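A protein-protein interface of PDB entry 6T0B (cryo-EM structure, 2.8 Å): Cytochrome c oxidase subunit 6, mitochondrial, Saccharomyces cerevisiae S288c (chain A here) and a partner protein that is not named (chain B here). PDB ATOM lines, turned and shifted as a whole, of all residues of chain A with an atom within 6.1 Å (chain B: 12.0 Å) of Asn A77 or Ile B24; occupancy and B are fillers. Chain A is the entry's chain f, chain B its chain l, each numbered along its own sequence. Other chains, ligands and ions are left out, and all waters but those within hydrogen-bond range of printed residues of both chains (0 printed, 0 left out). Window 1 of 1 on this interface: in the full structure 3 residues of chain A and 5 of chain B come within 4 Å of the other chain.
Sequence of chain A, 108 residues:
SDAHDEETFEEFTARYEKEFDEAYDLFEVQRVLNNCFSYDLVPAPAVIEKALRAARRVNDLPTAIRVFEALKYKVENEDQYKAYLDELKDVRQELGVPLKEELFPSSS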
ATOM      1  N   LYS A  72       2.926   1.106   0.184  1.00  0.00           N
ATOM      2  CA  LYS A  72       1.931   0.104  -0.179  1.00  0.00           C
ATOM      3  C   LYS A  72       2.209  -0.464  -1.559  1.00  0.00           C
ATOM      4  O   LYS A  72       2.150  -1.679  -1.758  1.00  0.00           O
ATOM      5  CB  LYS A  72       0.538   0.718  -0.134  1.00  0.00           C
ATOM      6  CG  LYS A  72      -0.574  -0.291  -0.233  1.00  0.00           C
ATOM      7  CD  LYS A  72      -1.924   0.366  -0.099  1.00  0.00           C
ATOM      8  CE  LYS A  72      -3.014  -0.670  -0.043  1.00  0.00           C
ATOM      9  NZ  LYS A  72      -4.327  -0.066   0.276  1.00  0.00           N
ATOM     10  N   VAL A  75       5.922  -2.602  -1.104  1.00  0.00           N
ATOM     11  CA  VAL A  75       6.125  -3.881  -0.435  1.00  0.00           C
ATOM     12  C   VAL A  75       5.556  -5.013  -1.276  1.00  0.00           C
ATOM     13  O   VAL A  75       4.762  -4.813  -2.194  1.00  0.00           O
ATOM     14  CB  VAL A  75       5.509  -3.889   0.967  1.00  0.00           C
ATOM     15  CG1 VAL A  75       6.186  -2.895   1.848  1.00  0.00           C
ATOM     16  CG2 VAL A  75       4.044  -3.608   0.874  1.00  0.00           C
ATOM     17  N   GLU A  76       5.959  -6.231  -0.930  1.00  0.00           N
ATOM     18  CA  GLU A  76       5.543  -7.409  -1.678  1.00  0.00           C
ATOM     19  C   GLU A  76       4.179  -7.937  -1.252  1.00  0.00           C
ATOM     20  O   GLU A  76       3.433  -8.445  -2.093  1.00  0.00           O
ATOM     21  CB  GLU A  76       6.570  -8.517  -1.511  1.00  0.00           C
ATOM     22  CG  GLU A  76       7.921  -8.232  -2.090  1.00  0.00           C
ATOM     23  CD  GLU A  76       8.762  -9.483  -2.158  1.00  0.00           C
ATOM     24  OE1 GLU A  76       8.327 -10.512  -1.607  1.00  0.00           O
ATOM     25  OE2 GLU A  76       9.853  -9.449  -2.762  1.00  0.00           O
ATOM     26  N   ASN A  77       3.846  -7.851   0.031  1.00  0.00           N
ATOM     27  CA  ASN A  77       2.632  -8.424   0.591  1.00  0.00           C
ATOM     28  C   ASN A  77       1.707  -7.315   1.056  1.00  0.00           C
ATOM     29  O   ASN A  77       1.950  -6.136   0.828  1.00  0.00           O
ATOM     30  CB  ASN A  77       2.942  -9.342   1.767  1.00  0.00           C
ATOM     31  CG  ASN A  77       3.880 -10.445   1.411  1.00  0.00           C
ATOM     32  OD1 ASN A  77       4.595 -10.950   2.264  1.00  0.00           O
ATOM     33  ND2 ASN A  77       3.877 -10.845   0.152  1.00  0.00           N
ATOM     34  N   GLU A  78       0.621  -7.708   1.707  1.00  0.00           N
ATOM     35  CA  GLU A  78      -0.124  -6.776   2.530  1.00  0.00           C
ATOM     36  C   GLU A  78       0.199  -6.937   4.002  1.00  0.00           C
ATOM     37  O   GLU A  78      -0.078  -6.026   4.788  1.00  0.00           O
ATOM     38  CB  GLU A  78      -1.634  -6.920   2.299  1.00  0.00           C
ATOM     39  CG  GLU A  78      -2.217  -8.316   2.473  1.00  0.00           C
ATOM     40  CD  GLU A  78      -2.779  -8.556   3.863  1.00  0.00           C
ATOM     41  OE1 GLU A  78      -2.851  -7.590   4.650  1.00  0.00           O
ATOM     42  OE2 GLU A  78      -3.179  -9.704   4.155  1.00  0.00           O
ATOM     43  N   ASP A  79       0.829  -8.042   4.381  1.00  0.00           N
ATOM     44  CA  ASP A  79       1.283  -8.181   5.751  1.00  0.00           C
ATOM     45  C   ASP A  79       2.601  -7.471   6.009  1.00  0.00           C
ATOM     46  O   ASP A  79       2.845  -7.065   7.143  1.00  0.00           O
ATOM     47  CB  ASP A  79       1.391  -9.651   6.120  1.00  0.00           C
ATOM     48  CG  ASP A  79       0.115 -10.403   5.842  1.00  0.00           C
ATOM     49  OD1 ASP A  79       0.185 -11.528   5.305  1.00  0.00           O
ATOM     50  OD2 ASP A  79      -0.967  -9.863   6.153  1.00  0.00           O
ATOM     51  N   GLN A  80       3.441  -7.280   4.992  1.00  0.00           N
ATOM     52  CA  GLN A  80       4.571  -6.372   5.150  1.00  0.00           C
ATOM     53  C   GLN A  80       4.094  -4.941   5.323  1.00  0.00           C
ATOM     54  O   GLN A  80       4.660  -4.181   6.115  1.00  0.00           O
ATOM     55  CB  GLN A  80       5.487  -6.470   3.944  1.00  0.00           C
ATOM     56  CG  GLN A  80       5.913  -7.854   3.635  1.00  0.00           C
ATOM     57  CD  GLN A  80       6.665  -7.923   2.350  1.00  0.00           C
ATOM     58  OE1 GLN A  80       6.585  -7.017   1.538  1.00  0.00           O
ATOM     59  NE2 GLN A  80       7.427  -8.987   2.160  1.00  0.00           N
ATOM     60  N   TYR A  81       3.052  -4.566   4.583  1.00  0.00           N
ATOM     61  CA  TYR A  81       2.434  -3.263   4.751  1.00  0.00           C
ATOM     62  C   TYR A  81       1.842  -3.117   6.139  1.00  0.00           C
ATOM     63  O   TYR A  81       1.973  -2.064   6.771  1.00  0.00           O
ATOM     64  CB  TYR A  81       1.361  -3.076   3.689  1.00  0.00           C
ATOM     65  CG  TYR A  81       0.670  -1.748   3.731  1.00  0.00           C
ATOM     66  CD1 TYR A  81       1.350  -0.600   3.429  1.00  0.00           C
ATOM     67  CD2 TYR A  81      -0.662  -1.649   4.050  1.00  0.00           C
ATOM     68  CE1 TYR A  81       0.738   0.618   3.460  1.00  0.00           C
ATOM     69  CE2 TYR A  81      -1.289  -0.435   4.076  1.00  0.00           C
ATOM     70  CZ  TYR A  81      -0.583   0.697   3.779  1.00  0.00           C
ATOM     71  OH  TYR A  81      -1.191   1.926   3.804  1.00  0.00           O
ATOM     72  N   ALA A  83       2.892  -4.724   8.782  1.00  0.00           N
ATOM     73  CA  ALA A  83       4.018  -4.645   9.704  1.00  0.00           C
ATOM     74  C   ALA A  83       4.610  -3.242   9.742  1.00  0.00           C
ATOM     75  O   ALA A  83       5.062  -2.786  10.794  1.00  0.00           O
ATOM     76  CB  ALA A  83       5.085  -5.660   9.309  1.00  0.00           C
ATOM     77  N   GLY B  22      13.860 -13.751   8.762  1.00  0.00           N
ATOM     78  CA  GLY B  22      12.550 -13.213   9.072  1.00  0.00           C
ATOM     79  C   GLY B  22      11.489 -13.661   8.092  1.00  0.00           C
ATOM     80  O   GLY B  22      10.642 -14.483   8.441  1.00  0.00           O
ATOM     81  N   ARG B  23      11.553 -13.100   6.881  1.00  0.00           N
ATOM     82  CA  ARG B  23      10.684 -13.425   5.748  1.00  0.00           C
ATOM     83  C   ARG B  23       9.209 -13.254   6.120  1.00  0.00           C
ATOM     84  O   ARG B  23       8.441 -14.208   6.239  1.00  0.00           O
ATOM     85  CB  ARG B  23      10.976 -14.830   5.210  1.00  0.00           C
ATOM     86  CG  ARG B  23      10.468 -15.067   3.797  1.00  0.00           C
ATOM     87  CD  ARG B  23      10.819 -13.916   2.871  1.00  0.00           C
ATOM     88  NE  ARG B  23       9.949 -13.879   1.704  1.00  0.00           N
ATOM     89  CZ  ARG B  23       8.758 -13.302   1.683  1.00  0.00           C
ATOM     90  NH1 ARG B  23       8.294 -12.707   2.769  1.00  0.00           N
ATOM     91  NH2 ARG B  23       8.031 -13.310   0.579  1.00  0.00           N
ATOM     92  N   ILE B  24       8.859 -11.990   6.344  1.00  0.00           N
ATOM     93  CA  ILE B  24       7.529 -11.633   6.813  1.00  0.00           C
ATOM     94  C   ILE B  24       6.503 -11.828   5.702  1.00  0.00           C
ATOM     95  O   ILE B  24       6.745 -11.510   4.531  1.00  0.00           O
ATOM     96  CB  ILE B  24       7.541 -10.193   7.359  1.00  0.00           C
ATOM     97  CG1 ILE B  24       6.187  -9.805   7.940  1.00  0.00           C
ATOM     98  CG2 ILE B  24       8.063  -9.192   6.339  1.00  0.00           C
ATOM     99  CD1 ILE B  24       5.903 -10.470   9.275  1.00  0.00           C
ATOM    100  N   GLY B  25       5.376 -12.424   6.056  1.00  0.00           N
ATOM    101  CA  GLY B  25       4.245 -12.510   5.164  1.00  0.00           C
ATOM    102  C   GLY B  25       4.191 -13.799   4.376  1.00  0.00           C
ATOM    103  O   GLY B  25       4.875 -14.784   4.656  1.00  0.00           O
ATOM    104  N   GLU B  26       3.327 -13.767   3.366  1.00  0.00           N
ATOM    105  CA  GLU B  26       3.115 -14.866   2.436  1.00  0.00           C
ATOM    106  C   GLU B  26       4.379 -15.143   1.629  1.00  0.00           C
ATOM    107  O   GLU B  26       5.214 -14.259   1.428  1.00  0.00           O
ATOM    108  CB  GLU B  26       1.953 -14.499   1.517  1.00  0.00           C
ATOM    109  CG  GLU B  26       1.382 -15.562   0.636  1.00  0.00           C
ATOM    110  CD  GLU B  26       0.482 -14.966  -0.424  1.00  0.00           C
ATOM    111  OE1 GLU B  26       0.926 -14.827  -1.583  1.00  0.00           O
ATOM    112  OE2 GLU B  26      -0.675 -14.629  -0.098  1.00  0.00           O
ATOM    113  N   SER B  27       4.520 -16.387   1.178  1.00  0.00           N
ATOM    114  CA  SER B  27       5.718 -16.804   0.470  1.00  0.00           C
ATOM    115  C   SER B  27       5.785 -16.171  -0.908  1.00  0.00           C
ATOM    116  O   SER B  27       4.762 -15.842  -1.515  1.00  0.00           O
ATOM    117  CB  SER B  27       5.750 -18.314   0.328  1.00  0.00           C
ATOM    118  OG  SER B  27       6.904 -18.698  -0.383  1.00  0.00           O
ATOM    119  N   TRP B  28       7.011 -16.005  -1.410  1.00  0.00           N
ATOM    120  CA  TRP B  28       7.170 -15.356  -2.701  1.00  0.00           C
ATOM    121  C   TRP B  28       6.734 -16.238  -3.851  1.00  0.00           C
ATOM    122  O   TRP B  28       6.301 -15.706  -4.877  1.00  0.00           O
ATOM    123  CB  TRP B  28       8.607 -14.878  -2.915  1.00  0.00           C
ATOM    124  CG  TRP B  28       9.674 -15.899  -2.818  1.00  0.00           C
ATOM    125  CD1 TRP B  28      10.369 -16.247  -1.704  1.00  0.00           C
ATOM    126  CD2 TRP B  28      10.226 -16.664  -3.889  1.00  0.00           C
ATOM    127  NE1 TRP B  28      11.304 -17.201  -2.005  1.00  0.00           N
ATOM    128  CE2 TRP B  28      11.235 -17.478  -3.343  1.00  0.00           C
ATOM    129  CE3 TRP B  28       9.948 -16.761  -5.254  1.00  0.00           C
ATOM    130  CZ2 TRP B  28      11.968 -18.372  -4.113  1.00  0.00           C
ATOM    131  CZ3 TRP B  28      10.674 -17.647  -6.014  1.00  0.00           C
ATOM    132  CH2 TRP B  28      11.673 -18.442  -5.444  1.00  0.00           C
ATOM    133  N   VAL B  29       6.778 -17.559  -3.683  1.00  0.00           N
ATOM    134  CA  VAL B  29       6.261 -18.440  -4.715  1.00  0.00           C
ATOM    135  C   VAL B  29       4.755 -18.288  -4.842  1.00  0.00           C
ATOM    136  O   VAL B  29       4.236 -18.258  -5.955  1.00  0.00           O
ATOM    137  CB  VAL B  29       6.695 -19.897  -4.466  1.00  0.00           C
ATOM    138  CG1 VAL B  29       8.201 -20.007  -4.558  1.00  0.00           C
ATOM    139  CG2 VAL B  29       6.243 -20.413  -3.118  1.00  0.00           C
ATOM    140  N   ILE B  30       4.048 -18.052  -3.742  1.00  0.00           N
ATOM    141  CA  ILE B  30       2.612 -17.824  -3.818  1.00  0.00           C
ATOM    142  C   ILE B  30       2.323 -16.440  -4.365  1.00  0.00           C
ATOM    143  O   ILE B  30       1.459 -16.272  -5.237  1.00  0.00           O
ATOM    144  CB  ILE B  30       1.973 -18.019  -2.436  1.00  0.00           C
ATOM    145  CG1 ILE B  30       2.399 -19.354  -1.833  1.00  0.00           C
ATOM    146  CG2 ILE B  30       0.478 -17.966  -2.551  1.00  0.00           C
ATOM    147  CD1 ILE B  30       2.036 -20.543  -2.676  1.00  0.00           C
ATOM    148  N   THR B  31       3.089 -15.452  -3.900  1.00  0.00           N
ATOM    149  CA  THR B  31       2.861 -14.061  -4.264  1.00  0.00           C
ATOM    150  C   THR B  31       3.078 -13.823  -5.751  1.00  0.00           C
ATOM    151  O   THR B  31       2.321 -13.079  -6.385  1.00  0.00           O
ATOM    152  CB  THR B  31       3.796 -13.170  -3.443  1.00  0.00           C
ATOM    153  OG1 THR B  31       3.582 -13.400  -2.049  1.00  0.00           O
ATOM    154  CG2 THR B  31       3.551 -11.707  -3.729  1.00  0.00           C
ATOM    155  N   GLU B  32       4.051 -14.505  -6.344  1.00  0.00           N
ATOM    156  CA  GLU B  32       4.299 -14.328  -7.759  1.00  0.00           C
ATOM    157  C   GLU B  32       3.652 -15.394  -8.621  1.00  0.00           C
ATOM    158  O   GLU B  32       3.461 -15.152  -9.810  1.00  0.00           O
ATOM    159  CB  GLU B  32       5.805 -14.277  -8.029  1.00  0.00           C
ATOM    160  CG  GLU B  32       6.330 -12.849  -8.065  1.00  0.00           C
ATOM    161  CD  GLU B  32       7.830 -12.770  -7.952  1.00  0.00           C
ATOM    162  OE1 GLU B  32       8.513 -13.713  -8.403  1.00  0.00           O
ATOM    163  OE2 GLU B  32       8.328 -11.768  -7.396  1.00  0.00           O
ATOM    164  N   GLY B  33       3.275 -16.545  -8.067  1.00  0.00           N
ATOM    165  CA  GLY B  33       2.489 -17.488  -8.835  1.00  0.00           C
ATOM    166  C   GLY B  33       1.092 -16.979  -9.097  1.00  0.00           C
ATOM    167  O   GLY B  33       0.594 -17.073 -10.221  1.00  0.00           O
ATOM    168  N   ARG B  34       0.463 -16.369  -8.090  1.00  0.00           N
ATOM    169  CA  ARG B  34      -0.877 -15.835  -8.306  1.00  0.00           C
ATOM    170  C   ARG B  34      -0.898 -14.591  -9.189  1.00  0.00           C
ATOM    171  O   ARG B  34      -1.983 -14.148  -9.573  1.00  0.00           O
ATOM    172  CB  ARG B  34      -1.555 -15.546  -6.965  1.00  0.00           C
ATOM    173  CG  ARG B  34      -1.297 -14.178  -6.385  1.00  0.00           C
ATOM    174  CD  ARG B  34      -2.178 -13.957  -5.188  1.00  0.00           C
ATOM    175  NE  ARG B  34      -2.016 -15.034  -4.228  1.00  0.00           N
ATOM    176  CZ  ARG B  34      -2.991 -15.500  -3.464  1.00  0.00           C
ATOM    177  NH1 ARG B  34      -4.203 -14.974  -3.545  1.00  0.00           N
ATOM    178  NH2 ARG B  34      -2.754 -16.487  -2.618  1.00  0.00           N
ATOM    179  N   ARG B  35       0.257 -14.031  -9.535  1.00  0.00           N
ATOM    180  CA  ARG B  35       0.369 -12.971 -10.527  1.00  0.00           C
ATOM    181  C   ARG B  35       0.769 -13.486 -11.904  1.00  0.00           C
ATOM    182  O   ARG B  35       0.216 -13.047 -12.913  1.00  0.00           O
ATOM    183  CB  ARG B  35       1.387 -11.931 -10.056  1.00  0.00           C
ATOM    184  CG  ARG B  35       1.704 -10.852 -11.049  1.00  0.00           C
ATOM    185  CD  ARG B  35       2.905 -10.064 -10.601  1.00  0.00           C
ATOM    186  NE  ARG B  35       4.151 -10.781 -10.827  1.00  0.00           N
ATOM    187  CZ  ARG B  35       4.814 -10.771 -11.976  1.00  0.00           C
ATOM    188  NH1 ARG B  35       4.345 -10.086 -13.006  1.00  0.00           N
ATOM    189  NH2 ARG B  35       5.944 -11.446 -12.099  1.00  0.00           N
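The side-chain amide nitrogen (ND2) of Asn A77 is in hydrogen-bond range of the side-chain hydroxyl (OG1) of Thr B31 (3.4 Å). N of Glu B26 sits at hydrogen-bond distance from OD1 of Asn A77, 3.3 Å away. The guanidinium group of Arg B23 is in salt-bridge range of the side-chain carboxylate of Glu A76 (3.6 Å). OD1 of Asn A77 sits close to O of Ile B24, at 3.2 Å.
The guanidinium group (NH2) of Arg B23 lies within hydrogen-bond range of the backbone carbonyl oxygen (O) of Glu B26 (3.1 Å). The side-chain carboxylate (OE1) of Glu B26 lies within hydrogen-bond range of the side-chain hydroxyl (OG1) of Thr B31 (3.1 Å). The backbone NH of Asn A77 lies within hydrogen-bond range of the side-chain amide oxygen of Gln A80 (3.2 Å). The backbone carbonyl oxygen (O) of Ser B27 is in hydrogen-bond range of the side-chain hydroxyl (OG1) of Thr B31. The guanidinium group of Arg B34 is in salt-bridge range of the side-chain carboxylate of Glu B26 (3.8 Å). N of Glu A76 is in hydrogen-bond range of OE1 of Gln A80.
Among the printed residues, merely in contact across the chains: Asn A77 with Gly B25 (3.3 Å), Gln A80 with Ile B24 (3.5 Å), Glu A76 with Thr B31 (3.7 Å) and Gln A80 with Arg B23 (3.9 Å).
Val A75 touches none of the printed residues of chain B. Asn A77 touches four residues of chain B. Glu A78 touches none of the printed residues of chain B. Asp A79 touches none of the printed residues of chain B. Gln A80 touches two residues of chain B. No residue of chain B comes within 4 Å of Ala A83. Printed residues of chain A within 4 Å of Arg B23: Glu A76 and Gln A80. Ile B24 touches two residues of chain A. Of the printed residues of chain A, Gly B25 touches Asn A77. Of the printed residues of chain A, Glu B26 touches Asn A77. Printed residues of chain A within 4 Å of Thr B31: Glu A76 (3.7 Å) and Asn A77 (3.4 Å). Arg B35 touches none of the printed residues of chain A.
Among the printed residues, 8 pairs touch across the chains. Among the printed residues, Asp or Glu carboxylates within 4 Å of a Lys or Arg side-chain nitrogen of the other chain: Glu A76 with Arg B23.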
